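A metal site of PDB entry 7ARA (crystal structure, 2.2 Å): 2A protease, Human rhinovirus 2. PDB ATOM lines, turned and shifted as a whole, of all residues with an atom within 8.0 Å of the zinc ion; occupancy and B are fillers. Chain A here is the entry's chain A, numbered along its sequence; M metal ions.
NH1 of Arg 134 lies within hydrogen-bond range of O of Cys 54, at 3.3 Å.
Within 4 Å of the zinc ion: Cys 52, Cys 54, Cys 112 and His 114. Along chain A the residues within 4 Å of the zinc ion span positions 52 to 114. The nearest printed residue that does not touch the zinc ion is Asp 53 (4.4 Å).
ND1 of His 114 is bound to the zinc ion, 2.1 Å away. The side-chain sulfur (SG) of Cys 54 binds the zinc ion (2.2 Å). The side-chain sulfur (SG) of Cys 52 binds the zinc ion (2.4 Å). SG of Cys 112 is bound to the zinc ion. The zinc ion has four donor atoms within binding distance.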
ATOM      1  N   PRO A  50      17.509  31.516 -19.069  1.00  0.00           N
ATOM      2  CA  PRO A  50      18.712  31.723 -19.879  1.00  0.00           C
ATOM      3  C   PRO A  50      18.439  32.531 -21.138  1.00  0.00           C
ATOM      4  O   PRO A  50      17.285  32.664 -21.534  1.00  0.00           O
ATOM      5  CB  PRO A  50      19.129  30.301 -20.245  1.00  0.00           C
ATOM      6  CG  PRO A  50      17.835  29.585 -20.340  1.00  0.00           C
ATOM      7  CD  PRO A  50      16.960  30.166 -19.253  1.00  0.00           C
ATOM      8  N   SER A  51      19.498  33.047 -21.741  1.00  0.00           N
ATOM      9  CA  SER A  51      19.391  33.750 -23.012  1.00  0.00           C
ATOM     10  C   SER A  51      20.025  32.905 -24.112  1.00  0.00           C
ATOM     11  O   SER A  51      21.032  33.292 -24.689  1.00  0.00           O
ATOM     12  CB  SER A  51      20.072  35.113 -22.929  1.00  0.00           C
ATOM     13  OG  SER A  51      21.397  34.988 -22.417  1.00  0.00           O
ATOM     14  N   CYS A  52      19.425  31.754 -24.387  1.00  0.00           N
ATOM     15  CA  CYS A  52      20.075  30.784 -25.245  1.00  0.00           C
ATOM     16  C   CYS A  52      19.220  30.281 -26.396  1.00  0.00           C
ATOM     17  O   CYS A  52      18.371  30.982 -26.941  1.00  0.00           O
ATOM     18  CB  CYS A  52      20.552  29.590 -24.407  1.00  0.00           C
ATOM     19  SG  CYS A  52      19.208  28.605 -23.688  1.00  0.00           S
ATOM     20  N   ASP A  53      19.453  29.015 -26.740  1.00  0.00           N
ATOM     21  CA  ASP A  53      19.125  28.482 -28.055  1.00  0.00           C
ATOM     22  C   ASP A  53      18.337  27.175 -28.000  1.00  0.00           C
ATOM     23  O   ASP A  53      17.576  26.864 -28.922  1.00  0.00           O
ATOM     24  CB  ASP A  53      20.418  28.257 -28.824  1.00  0.00           C
ATOM     25  CG  ASP A  53      21.447  27.467 -28.011  1.00  0.00           C
ATOM     26  OD1 ASP A  53      22.249  28.102 -27.300  1.00  0.00           O
ATOM     27  OD2 ASP A  53      21.434  26.225 -28.074  1.00  0.00           O
ATOM     28  N   CYS A  54      18.536  26.425 -26.917  1.00  0.00           N
ATOM     29  CA  CYS A  54      18.123  25.029 -26.791  1.00  0.00           C
ATOM     30  C   CYS A  54      16.748  24.654 -27.358  1.00  0.00           C
ATOM     31  O   CYS A  54      15.794  25.433 -27.283  1.00  0.00           O
ATOM     32  CB  CYS A  54      18.174  24.602 -25.320  1.00  0.00           C
ATOM     33  SG  CYS A  54      19.839  24.582 -24.629  1.00  0.00           S
ATOM     34  N   THR A  55      16.664  23.462 -27.917  1.00  0.00           N
ATOM     35  CA  THR A  55      15.417  22.934 -28.462  1.00  0.00           C
ATOM     36  C   THR A  55      15.101  21.597 -27.803  1.00  0.00           C
ATOM     37  O   THR A  55      13.995  21.097 -27.879  1.00  0.00           O
ATOM     38  CB  THR A  55      15.494  22.745 -29.980  1.00  0.00           C
ATOM     39  OG1 THR A  55      14.252  22.208 -30.455  1.00  0.00           O
ATOM     40  CG2 THR A  55      16.640  21.813 -30.339  1.00  0.00           C
ATOM     41  N   GLN A  56      16.125  21.054 -27.146  1.00  0.00           N
ATOM     42  CA  GLN A  56      16.061  19.761 -26.481  1.00  0.00           C
ATOM     43  C   GLN A  56      15.944  19.980 -24.980  1.00  0.00           C
ATOM     44  O   GLN A  56      16.888  20.450 -24.327  1.00  0.00           O
ATOM     45  CB  GLN A  56      17.293  18.927 -26.819  1.00  0.00           C
ATOM     46  CG  GLN A  56      17.492  17.702 -25.926  1.00  0.00           C
ATOM     47  CD  GLN A  56      18.883  17.078 -26.112  1.00  0.00           C
ATOM     48  OE1 GLN A  56      19.857  17.742 -26.460  1.00  0.00           O
ATOM     49  NE2 GLN A  56      18.955  15.781 -25.869  1.00  0.00           N
ATOM     50  N   ALA A  57      14.784  19.606 -24.441  1.00  0.00           N
ATOM     51  CA  ALA A  57      14.347  20.050 -23.118  1.00  0.00           C
ATOM     52  C   ALA A  57      13.509  19.022 -22.331  1.00  0.00           C
ATOM     53  O   ALA A  57      13.390  17.855 -22.727  1.00  0.00           O
ATOM     54  CB  ALA A  57      13.550  21.340 -23.278  1.00  0.00           C
ATOM     55  N   LEU A 111      11.996  23.321 -18.862  1.00  0.00           N
ATOM     56  CA  LEU A 111      13.409  23.577 -18.637  1.00  0.00           C
ATOM     57  C   LEU A 111      14.303  23.005 -19.725  1.00  0.00           C
ATOM     58  O   LEU A 111      13.979  21.989 -20.338  1.00  0.00           O
ATOM     59  CB  LEU A 111      13.867  23.006 -17.288  1.00  0.00           C
ATOM     60  CG  LEU A 111      13.260  23.565 -16.004  1.00  0.00           C
ATOM     61  CD1 LEU A 111      12.015  22.799 -15.619  1.00  0.00           C
ATOM     62  CD2 LEU A 111      14.297  23.522 -14.897  1.00  0.00           C
ATOM     63  N   CYS A 112      15.428  23.668 -19.956  1.00  0.00           N
ATOM     64  CA  CYS A 112      16.485  23.098 -20.787  1.00  0.00           C
ATOM     65  C   CYS A 112      17.701  22.915 -19.883  1.00  0.00           C
ATOM     66  O   CYS A 112      17.573  22.898 -18.657  1.00  0.00           O
ATOM     67  CB  CYS A 112      16.824  24.001 -21.969  1.00  0.00           C
ATOM     68  SG  CYS A 112      17.806  25.454 -21.563  1.00  0.00           S
ATOM     69  N   LYS A 113      18.881  22.777 -20.482  1.00  0.00           N
ATOM     70  CA  LYS A 113      20.082  22.482 -19.715  1.00  0.00           C
ATOM     71  C   LYS A 113      20.550  23.679 -18.888  1.00  0.00           C
ATOM     72  O   LYS A 113      21.279  23.521 -17.923  1.00  0.00           O
ATOM     73  CB  LYS A 113      21.203  22.027 -20.655  1.00  0.00           C
ATOM     74  CG  LYS A 113      20.692  21.459 -21.974  1.00  0.00           C
ATOM     75  CD  LYS A 113      21.425  20.179 -22.350  1.00  0.00           C
ATOM     76  CE  LYS A 113      20.798  19.546 -23.588  1.00  0.00           C
ATOM     77  NZ  LYS A 113      21.337  18.183 -23.856  1.00  0.00           N
ATOM     78  N   HIS A 114      20.101  24.873 -19.277  1.00  0.00           N
ATOM     79  CA  HIS A 114      20.591  26.114 -18.683  1.00  0.00           C
ATOM     80  C   HIS A 114      19.664  26.647 -17.601  1.00  0.00           C
ATOM     81  O   HIS A 114      20.116  27.298 -16.650  1.00  0.00           O
ATOM     82  CB  HIS A 114      20.782  27.184 -19.767  1.00  0.00           C
ATOM     83  CG  HIS A 114      21.592  26.722 -20.940  1.00  0.00           C
ATOM     84  ND1 HIS A 114      21.018  26.260 -22.106  1.00  0.00           N
ATOM     85  CD2 HIS A 114      22.930  26.650 -21.123  1.00  0.00           C
ATOM     86  CE1 HIS A 114      21.970  25.923 -22.953  1.00  0.00           C
ATOM     87  NE2 HIS A 114      23.139  26.153 -22.385  1.00  0.00           N
ATOM     88  N   GLY A 115      18.379  26.370 -17.747  1.00  0.00           N
ATOM     89  CA  GLY A 115      17.389  26.861 -16.809  1.00  0.00           C
ATOM     90  C   GLY A 115      15.991  26.766 -17.390  1.00  0.00           C
ATOM     91  O   GLY A 115      15.730  25.961 -18.284  1.00  0.00           O
ATOM     92  N   VAL A 116      15.085  27.604 -16.889  1.00  0.00           N
ATOM     93  CA  VAL A 116      13.700  27.533 -17.332  1.00  0.00           C
ATOM     94  C   VAL A 116      13.476  28.441 -18.527  1.00  0.00           C
ATOM     95  O   VAL A 116      13.921  29.589 -18.539  1.00  0.00           O
ATOM     96  CB  VAL A 116      12.733  27.918 -16.203  1.00  0.00           C
ATOM     97  CG1 VAL A 116      11.356  27.379 -16.505  1.00  0.00           C
ATOM     98  CG2 VAL A 116      13.230  27.355 -14.878  1.00  0.00           C
ATOM     99  N   ILE A 117      12.782  27.926 -19.530  1.00  0.00           N
ATOM    100  CA  ILE A 117      12.581  28.693 -20.755  1.00  0.00           C
ATOM    101  C   ILE A 117      11.109  28.836 -21.114  1.00  0.00           C
ATOM    102  O   ILE A 117      10.750  29.534 -22.052  1.00  0.00           O
ATOM    103  CB  ILE A 117      13.325  28.063 -21.939  1.00  0.00           C
ATOM    104  CG1 ILE A 117      12.808  26.640 -22.205  1.00  0.00           C
ATOM    105  CG2 ILE A 117      14.813  28.027 -21.674  1.00  0.00           C
ATOM    106  CD1 ILE A 117      13.589  25.912 -23.270  1.00  0.00           C
ATOM    107  N   ARG A 134      12.118  33.298 -22.893  1.00  0.00           N
ATOM    108  CA  ARG A 134      13.374  33.892 -23.334  1.00  0.00           C
ATOM    109  C   ARG A 134      13.121  35.150 -24.163  1.00  0.00           C
ATOM    110  O   ARG A 134      13.958  36.056 -24.204  1.00  0.00           O
ATOM    111  CB  ARG A 134      14.177  32.889 -24.154  1.00  0.00           C
ATOM    112  CG  ARG A 134      14.774  31.751 -23.337  1.00  0.00           C
ATOM    113  CD  ARG A 134      15.327  30.673 -24.245  1.00  0.00           C
ATOM    114  NE  ARG A 134      14.292  30.160 -25.139  1.00  0.00           N
ATOM    115  CZ  ARG A 134      14.443  29.126 -25.953  1.00  0.00           C
ATOM    116  NH1 ARG A 134      15.596  28.472 -25.977  1.00  0.00           N
ATOM    117  NH2 ARG A 134      13.442  28.725 -26.722  1.00  0.00           N
HETATM  118 ZN    ZN M   1      19.324  26.290 -23.267  1.00  0.00          ZN
